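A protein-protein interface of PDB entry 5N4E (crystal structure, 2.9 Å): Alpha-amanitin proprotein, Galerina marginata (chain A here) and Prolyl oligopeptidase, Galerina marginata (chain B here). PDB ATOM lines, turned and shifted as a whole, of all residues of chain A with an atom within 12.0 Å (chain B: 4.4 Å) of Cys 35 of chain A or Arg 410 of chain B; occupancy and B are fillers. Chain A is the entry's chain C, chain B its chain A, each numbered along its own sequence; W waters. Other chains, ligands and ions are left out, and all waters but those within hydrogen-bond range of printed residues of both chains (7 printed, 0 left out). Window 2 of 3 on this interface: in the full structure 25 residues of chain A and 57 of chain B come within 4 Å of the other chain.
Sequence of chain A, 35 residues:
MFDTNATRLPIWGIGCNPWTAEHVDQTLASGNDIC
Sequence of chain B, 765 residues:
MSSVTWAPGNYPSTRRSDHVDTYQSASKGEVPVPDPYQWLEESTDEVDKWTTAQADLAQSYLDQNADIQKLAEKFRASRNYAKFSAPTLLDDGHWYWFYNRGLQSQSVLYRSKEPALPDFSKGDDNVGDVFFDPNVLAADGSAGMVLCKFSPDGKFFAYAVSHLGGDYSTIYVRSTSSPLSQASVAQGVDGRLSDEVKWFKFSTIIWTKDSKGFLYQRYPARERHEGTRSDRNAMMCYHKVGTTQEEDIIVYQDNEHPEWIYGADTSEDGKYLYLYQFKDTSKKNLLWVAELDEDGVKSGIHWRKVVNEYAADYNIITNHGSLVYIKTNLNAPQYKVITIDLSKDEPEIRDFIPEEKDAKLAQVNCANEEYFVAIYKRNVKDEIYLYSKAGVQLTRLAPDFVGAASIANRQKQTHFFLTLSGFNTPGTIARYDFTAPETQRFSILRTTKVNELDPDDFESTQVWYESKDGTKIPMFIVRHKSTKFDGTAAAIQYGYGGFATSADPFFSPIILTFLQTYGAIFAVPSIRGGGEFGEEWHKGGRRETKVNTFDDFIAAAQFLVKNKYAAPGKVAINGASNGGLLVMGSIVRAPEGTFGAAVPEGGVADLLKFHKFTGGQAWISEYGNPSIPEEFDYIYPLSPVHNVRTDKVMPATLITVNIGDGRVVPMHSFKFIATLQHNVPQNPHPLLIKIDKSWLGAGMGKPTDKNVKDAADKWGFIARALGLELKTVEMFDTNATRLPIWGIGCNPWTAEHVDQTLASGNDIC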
ATOM      1  N   PHE A   2     -10.028  23.013   2.971  1.00  0.00           N
ATOM      2  CA  PHE A   2      -9.512  21.623   2.758  1.00  0.00           C
ATOM      3  C   PHE A   2      -8.967  21.439   1.340  1.00  0.00           C
ATOM      4  O   PHE A   2      -9.509  21.992   0.380  1.00  0.00           O
ATOM      5  CB  PHE A   2     -10.614  20.591   3.037  1.00  0.00           C
ATOM      6  CG  PHE A   2     -10.138  19.161   3.002  1.00  0.00           C
ATOM      7  CD1 PHE A   2      -9.516  18.593   4.110  1.00  0.00           C
ATOM      8  CD2 PHE A   2     -10.319  18.377   1.863  1.00  0.00           C
ATOM      9  CE1 PHE A   2      -9.082  17.275   4.084  1.00  0.00           C
ATOM     10  CE2 PHE A   2      -9.883  17.061   1.829  1.00  0.00           C
ATOM     11  CZ  PHE A   2      -9.264  16.509   2.940  1.00  0.00           C
ATOM     12  N   ALA A  29      -7.402  26.896  14.019  1.00  0.00           N
ATOM     13  CA  ALA A  29      -8.075  26.724  12.725  1.00  0.00           C
ATOM     14  C   ALA A  29      -9.026  25.512  12.641  1.00  0.00           C
ATOM     15  O   ALA A  29      -9.677  25.325  11.611  1.00  0.00           O
ATOM     16  CB  ALA A  29      -7.038  26.650  11.613  1.00  0.00           C
ATOM     17  N   SER A  30      -9.132  24.720  13.712  1.00  0.00           N
ATOM     18  CA  SER A  30      -9.901  23.458  13.690  1.00  0.00           C
ATOM     19  C   SER A  30     -11.418  23.609  13.545  1.00  0.00           C
ATOM     20  O   SER A  30     -12.097  22.638  13.193  1.00  0.00           O
ATOM     21  CB  SER A  30      -9.608  22.618  14.941  1.00  0.00           C
ATOM     22  OG  SER A  30      -9.936  23.318  16.126  1.00  0.00           O
ATOM     23  N   GLY A  31     -11.940  24.807  13.822  1.00  0.00           N
ATOM     24  CA  GLY A  31     -13.371  25.099  13.704  1.00  0.00           C
ATOM     25  C   GLY A  31     -13.746  25.892  12.461  1.00  0.00           C
ATOM     26  O   GLY A  31     -14.862  26.406  12.378  1.00  0.00           O
ATOM     27  N   ASN A  32     -12.828  25.984  11.496  1.00  0.00           N
ATOM     28  CA  ASN A  32     -13.028  26.816  10.303  1.00  0.00           C
ATOM     29  C   ASN A  32     -13.980  26.186   9.281  1.00  0.00           C
ATOM     30  O   ASN A  32     -14.701  26.914   8.591  1.00  0.00           O
ATOM     31  CB  ASN A  32     -11.686  27.153   9.623  1.00  0.00           C
ATOM     32  CG  ASN A  32     -10.875  28.196  10.381  1.00  0.00           C
ATOM     33  OD1 ASN A  32     -11.263  28.668  11.452  1.00  0.00           O
ATOM     34  ND2 ASN A  32      -9.733  28.564   9.813  1.00  0.00           N
ATOM     35  N   ASP A  33     -13.983  24.854   9.173  1.00  0.00           N
ATOM     36  CA  ASP A  33     -14.885  24.156   8.251  1.00  0.00           C
ATOM     37  C   ASP A  33     -15.411  22.841   8.841  1.00  0.00           C
ATOM     38  O   ASP A  33     -15.065  21.750   8.387  1.00  0.00           O
ATOM     39  CB  ASP A  33     -14.190  23.937   6.896  1.00  0.00           C
ATOM     40  CG  ASP A  33     -15.155  23.526   5.788  1.00  0.00           C
ATOM     41  OD1 ASP A  33     -14.704  22.831   4.856  1.00  0.00           O
ATOM     42  OD2 ASP A  33     -16.351  23.893   5.839  1.00  0.00           O
ATOM     43  N   ILE A  34     -16.266  22.978   9.853  1.00  0.00           N
ATOM     44  CA  ILE A  34     -16.957  21.841  10.490  1.00  0.00           C
ATOM     45  C   ILE A  34     -18.454  21.766  10.140  1.00  0.00           C
ATOM     46  O   ILE A  34     -19.172  20.930  10.687  1.00  0.00           O
ATOM     47  CB  ILE A  34     -16.767  21.835  12.033  1.00  0.00           C
ATOM     48  CG1 ILE A  34     -17.281  23.134  12.680  1.00  0.00           C
ATOM     49  CG2 ILE A  34     -15.301  21.607  12.373  1.00  0.00           C
ATOM     50  CD1 ILE A  34     -17.473  23.038  14.173  1.00  0.00           C
ATOM     51  N   CYS A  35     -18.924  22.638   9.246  1.00  0.00           N
ATOM     52  CA  CYS A  35     -20.297  22.571   8.738  1.00  0.00           C
ATOM     53  C   CYS A  35     -20.404  23.212   7.356  1.00  0.00           C
ATOM     54  O   CYS A  35     -20.229  24.418   7.196  1.00  0.00           O
ATOM     55  CB  CYS A  35     -21.268  23.250   9.707  1.00  0.00           C
ATOM     56  SG  CYS A  35     -23.004  22.992   9.277  1.00  0.00           S
ATOM     57  OXT CYS A  35     -20.664  22.539   6.361  1.00  0.00           O
ATOM     58  N   THR B  88     -18.638  28.200  15.221  1.00  0.00           N
ATOM     59  CA  THR B  88     -19.504  27.978  14.054  1.00  0.00           C
ATOM     60  C   THR B  88     -20.970  27.927  14.486  1.00  0.00           C
ATOM     61  O   THR B  88     -21.329  27.143  15.370  1.00  0.00           O
ATOM     62  CB  THR B  88     -19.160  26.654  13.333  1.00  0.00           C
ATOM     63  OG1 THR B  88     -17.755  26.603  13.046  1.00  0.00           O
ATOM     64  CG2 THR B  88     -19.951  26.521  12.028  1.00  0.00           C
ATOM     65  N   LEU B  89     -21.808  28.757  13.860  1.00  0.00           N
ATOM     66  CA  LEU B  89     -23.246  28.769  14.132  1.00  0.00           C
ATOM     67  C   LEU B  89     -23.947  27.689  13.311  1.00  0.00           C
ATOM     68  O   LEU B  89     -24.001  27.786  12.085  1.00  0.00           O
ATOM     69  CB  LEU B  89     -23.857  30.139  13.807  1.00  0.00           C
ATOM     70  CG  LEU B  89     -25.380  30.283  13.922  1.00  0.00           C
ATOM     71  CD1 LEU B  89     -25.847  29.986  15.334  1.00  0.00           C
ATOM     72  CD2 LEU B  89     -25.817  31.674  13.494  1.00  0.00           C
ATOM     73  N   LEU B  90     -24.482  26.674  13.986  1.00  0.00           N
ATOM     74  CA  LEU B  90     -25.311  25.655  13.332  1.00  0.00           C
ATOM     75  C   LEU B  90     -26.766  26.118  13.229  1.00  0.00           C
ATOM     76  O   LEU B  90     -27.157  27.114  13.847  1.00  0.00           O
ATOM     77  CB  LEU B  90     -25.216  24.315  14.074  1.00  0.00           C
ATOM     78  CG  LEU B  90     -23.824  23.673  14.194  1.00  0.00           C
ATOM     79  CD1 LEU B  90     -23.963  22.267  14.755  1.00  0.00           C
ATOM     80  CD2 LEU B  90     -23.068  23.648  12.869  1.00  0.00           C
ATOM     81  N   ASP B  91     -27.555  25.384  12.442  1.00  0.00           N
ATOM     82  CA  ASP B  91     -28.969  25.721  12.194  1.00  0.00           C
ATOM     83  C   ASP B  91     -29.914  25.470  13.381  1.00  0.00           C
ATOM     84  O   ASP B  91     -31.088  25.813  13.304  1.00  0.00           O
ATOM     85  CB  ASP B  91     -29.492  24.976  10.955  1.00  0.00           C
ATOM     86  CG  ASP B  91     -28.869  25.470   9.651  1.00  0.00           C
ATOM     87  OD1 ASP B  91     -27.906  26.268   9.680  1.00  0.00           O
ATOM     88  OD2 ASP B  91     -29.354  25.047   8.578  1.00  0.00           O
ATOM     89  N   LYS B 149     -17.541  16.804  10.635  1.00  0.00           N
ATOM     90  CA  LYS B 149     -18.433  17.634   9.832  1.00  0.00           C
ATOM     91  C   LYS B 149     -19.881  17.515  10.312  1.00  0.00           C
ATOM     92  O   LYS B 149     -20.478  16.440  10.233  1.00  0.00           O
ATOM     93  CB  LYS B 149     -18.326  17.236   8.352  1.00  0.00           C
ATOM     94  CG  LYS B 149     -18.434  18.404   7.385  1.00  0.00           C
ATOM     95  CD  LYS B 149     -17.147  19.210   7.333  1.00  0.00           C
ATOM     96  CE  LYS B 149     -17.153  20.175   6.158  1.00  0.00           C
ATOM     97  NZ  LYS B 149     -17.033  19.479   4.845  1.00  0.00           N
ATOM     98  N   PHE B 150     -20.428  18.615  10.829  1.00  0.00           N
ATOM     99  CA  PHE B 150     -21.864  18.712  11.107  1.00  0.00           C
ATOM    100  C   PHE B 150     -22.633  18.723   9.794  1.00  0.00           C
ATOM    101  O   PHE B 150     -22.133  19.233   8.787  1.00  0.00           O
ATOM    102  CB  PHE B 150     -22.207  19.990  11.881  1.00  0.00           C
ATOM    103  CG  PHE B 150     -21.833  19.950  13.335  1.00  0.00           C
ATOM    104  CD1 PHE B 150     -22.618  19.247  14.247  1.00  0.00           C
ATOM    105  CD2 PHE B 150     -20.713  20.638  13.803  1.00  0.00           C
ATOM    106  CE1 PHE B 150     -22.280  19.218  15.592  1.00  0.00           C
ATOM    107  CE2 PHE B 150     -20.376  20.612  15.146  1.00  0.00           C
ATOM    108  CZ  PHE B 150     -21.157  19.902  16.040  1.00  0.00           C
ATOM    109  N   SER B 151     -23.848  18.177   9.808  1.00  0.00           N
ATOM    110  CA  SER B 151     -24.746  18.277   8.658  1.00  0.00           C
ATOM    111  C   SER B 151     -25.207  19.734   8.494  1.00  0.00           C
ATOM    112  O   SER B 151     -25.151  20.504   9.460  1.00  0.00           O
ATOM    113  CB  SER B 151     -25.953  17.347   8.814  1.00  0.00           C
ATOM    114  OG  SER B 151     -26.669  17.626  10.001  1.00  0.00           O
ATOM    115  N   PRO B 152     -25.652  20.123   7.278  1.00  0.00           N
ATOM    116  CA  PRO B 152     -26.196  21.469   7.045  1.00  0.00           C
ATOM    117  C   PRO B 152     -27.334  21.863   7.993  1.00  0.00           C
ATOM    118  O   PRO B 152     -27.320  22.972   8.518  1.00  0.00           O
ATOM    119  CB  PRO B 152     -26.703  21.400   5.602  1.00  0.00           C
ATOM    120  CG  PRO B 152     -25.856  20.370   4.961  1.00  0.00           C
ATOM    121  CD  PRO B 152     -25.511  19.370   6.021  1.00  0.00           C
ATOM    122  N   ASN B 409     -16.512  30.614   7.722  1.00  0.00           N
ATOM    123  CA  ASN B 409     -17.906  31.028   7.538  1.00  0.00           C
ATOM    124  C   ASN B 409     -18.796  29.959   6.910  1.00  0.00           C
ATOM    125  O   ASN B 409     -18.316  28.940   6.407  1.00  0.00           O
ATOM    126  CB  ASN B 409     -17.975  32.318   6.700  1.00  0.00           C
ATOM    127  CG  ASN B 409     -17.815  32.079   5.210  1.00  0.00           C
ATOM    128  OD1 ASN B 409     -17.004  31.265   4.782  1.00  0.00           O
ATOM    129  ND2 ASN B 409     -18.584  32.808   4.411  1.00  0.00           N
ATOM    130  N   ARG B 410     -20.100  30.217   6.958  1.00  0.00           N
ATOM    131  CA  ARG B 410     -21.092  29.507   6.159  1.00  0.00           C
ATOM    132  C   ARG B 410     -21.743  30.549   5.252  1.00  0.00           C
ATOM    133  O   ARG B 410     -22.124  31.621   5.719  1.00  0.00           O
ATOM    134  CB  ARG B 410     -22.135  28.835   7.052  1.00  0.00           C
ATOM    135  CG  ARG B 410     -21.552  27.806   8.006  1.00  0.00           C
ATOM    136  CD  ARG B 410     -22.621  27.217   8.904  1.00  0.00           C
ATOM    137  NE  ARG B 410     -23.565  26.378   8.162  1.00  0.00           N
ATOM    138  CZ  ARG B 410     -24.730  25.918   8.631  1.00  0.00           C
ATOM    139  NH1 ARG B 410     -25.148  26.204   9.865  1.00  0.00           N
ATOM    140  NH2 ARG B 410     -25.493  25.161   7.848  1.00  0.00           N
ATOM    141  N   GLN B 411     -21.860  30.221   3.964  1.00  0.00           N
ATOM    142  CA  GLN B 411     -22.275  31.171   2.920  1.00  0.00           C
ATOM    143  C   GLN B 411     -23.553  31.953   3.233  1.00  0.00           C
ATOM    144  O   GLN B 411     -23.593  33.176   3.069  1.00  0.00           O
ATOM    145  CB  GLN B 411     -22.450  30.438   1.580  1.00  0.00           C
ATOM    146  CG  GLN B 411     -22.815  31.341   0.403  1.00  0.00           C
ATOM    147  CD  GLN B 411     -22.871  30.605  -0.913  1.00  0.00           C
ATOM    148  OE1 GLN B 411     -21.907  29.950  -1.305  1.00  0.00           O
ATOM    149  NE2 GLN B 411     -23.998  30.711  -1.609  1.00  0.00           N
ATOM    150  N   LYS B 412     -24.585  31.243   3.680  1.00  0.00           N
ATOM    151  CA  LYS B 412     -25.910  31.843   3.876  1.00  0.00           C
ATOM    152  C   LYS B 412     -26.009  32.819   5.056  1.00  0.00           C
ATOM    153  O   LYS B 412     -26.943  33.623   5.112  1.00  0.00           O
ATOM    154  CB  LYS B 412     -26.973  30.742   4.008  1.00  0.00           C
ATOM    155  CG  LYS B 412     -26.983  29.989   5.329  1.00  0.00           C
ATOM    156  CD  LYS B 412     -27.803  28.712   5.220  1.00  0.00           C
ATOM    157  CE  LYS B 412     -28.076  28.106   6.587  1.00  0.00           C
ATOM    158  NZ  LYS B 412     -28.618  26.720   6.495  1.00  0.00           N
ATOM    159  N   GLN B 413     -25.059  32.751   5.990  1.00  0.00           N
ATOM    160  CA  GLN B 413     -25.113  33.539   7.220  1.00  0.00           C
ATOM    161  C   GLN B 413     -24.597  34.957   7.017  1.00  0.00           C
ATOM    162  O   GLN B 413     -23.805  35.217   6.118  1.00  0.00           O
ATOM    163  CB  GLN B 413     -24.312  32.844   8.320  1.00  0.00           C
ATOM    164  CG  GLN B 413     -24.811  31.443   8.650  1.00  0.00           C
ATOM    165  CD  GLN B 413     -24.027  30.775   9.760  1.00  0.00           C
ATOM    166  OE1 GLN B 413     -22.831  31.013   9.928  1.00  0.00           O
ATOM    167  NE2 GLN B 413     -24.698  29.917  10.520  1.00  0.00           N
HETATM  168  O   HOH W   1     -15.656  28.160   6.351  1.00  0.00           O
HETATM  169  O   HOH W   2     -25.894  23.217  10.728  1.00  0.00           O
HETATM  170  O   HOH W   3     -22.002  19.812   6.114  1.00  0.00           O
HETATM  171  O   HOH W   4     -19.282  26.061   5.247  1.00  0.00           O
HETATM  172  O   HOH W   5     -16.217  25.868  15.201  1.00  0.00           O
HETATM  173  O   HOH W   6     -16.815  25.816  10.730  1.00  0.00           O
HETATM  174  O   HOH W   7     -22.604  25.166   5.884  1.00  0.00           O
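The backbone carbonyl oxygen (O) of Gly 31 of chain A sits at hydrogen-bond distance from the side-chain hydroxyl (OG1) of Thr 88 of chain B. The backbone carbonyl oxygen (O) of Ile 34 of chain A lies within hydrogen-bond range of the backbone NH (N) of Phe 150 of chain B (2.6 Å). O of Ser 151 of chain B is in hydrogen-bond range of SG of Cys 35 of chain A (3.3 Å). The guanidinium group (NE) of Arg 410 of chain B is in salt-bridge range of the chain-end carboxylate (O) of Cys 35 of chain A (3.99 Å).
NH1 of Arg 410 of chain B is in hydrogen-bond range of O of Leu 89 of chain B. The side-chain carboxylate (OD1) of Asp 91 of chain B is in salt-bridge range of the guanidinium group (NH1) of Arg 410 of chain B. The guanidinium group of Arg 410 of chain B lies within hydrogen-bond range of the backbone carbonyl oxygen of Pro 152 of chain B (2.9 Å).
Among the printed residues, pairs that only touch across the chains: Asp 33 of chain A with Lys 149 of chain B (3.4 Å), Ile 34 of chain A with Lys 149 of chain B (3.5 Å), Ile 34 of chain A with Thr 88 of chain B (3.5 Å), Cys 35 of chain A with Leu 90 of chain B (3.7 Å) and Cys 35 of chain A with Phe 150 of chain B (3.8 Å).
Of chain B, only Leu 90, Phe 150, Ser 151 and Arg 410 come within 4 Å of Cys 35 of chain A. Arg 410 of chain B touches one residue of chain A. Thr 88 of chain B touches two residues of chain A. Leu 89 of chain B touches none of the printed residues of chain A. Of chain A, only Cys 35 comes within 4 Å of Leu 90 of chain B. Asp 91 of chain B touches none of the printed residues of chain A. Lys 149 of chain B touches two residues of chain A. Of chain A, only Ile 34 and Cys 35 come within 4 Å of Phe 150 of chain B. Ser 151 of chain B touches just one residue of chain A: Cys 35 (3.3 Å). No residue of chain A comes within 4 Å of Pro 152 of chain B. No residue of chain A comes within 4 Å of Asn 409 of chain B. No residue of chain A comes within 4 Å of Gln 411 of chain B. No residue of chain A comes within 4 Å of Lys 412 of chain B. No residue of chain A comes within 4 Å of Gln 413 of chain B. Printed residues of chain B within 4 Å of Asp 33 of chain A: Lys 149. Of the printed residues of chain B, Ile 34 of chain A touches Thr 88 (3.5 Å), Lys 149 (3.5 Å) and Phe 150 (2.6 Å). Of the printed residues of chain B, Gly 31 of chain A touches Thr 88. Asn 32 of chain A touches none of the printed residues of chain B. The nearest residue of chain A that does not touch Arg 410 of chain B is Asn 32 of chain A (6.5 Å).
Of the 13 printed residues of chain B, 6 touch a printed residue of chain A. Hydrophobic or aromatic side chains of chain B that line the printed part of chain A: Leu 90 and Phe 150. Hydrophobic or aromatic side chains of chain A that line the printed part of chain B: Ile 34.
Water W6 lies within hydrogen-bond range of OG1 of Thr 88 of chain B (2.6 Å), O of Gly 31 of chain A (2.6 Å), N of Ile 34 of chain A (3.0 Å), O of Asn 32 of chain A (3.2 Å) and N of Asp 33 of chain A (3.4 Å). Water W4 lies within hydrogen-bond range of O of Cys 35 of chain A and O of Asn 409 of chain B. Water W1 lies within hydrogen-bond range of the backbone carbonyl oxygen (O) of Asn 32 of chain A (2.7 Å) and the backbone carbonyl oxygen (O) of Asn 409 of chain B (2.8 Å). Water W3 bridges the backbone carbonyl oxygen of Phe 150 of chain B and the chain-end carboxylate of Cys 35 of chain A. Water W5 lies within hydrogen-bond range of the side-chain hydroxyl of Thr 88 of chain B (2.7 Å) and the backbone carbonyl oxygen of Gly 31 of chain A (3.2 Å). Water W7 bridges NE of Arg 410 of chain B and O of Cys 35 of chain A.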
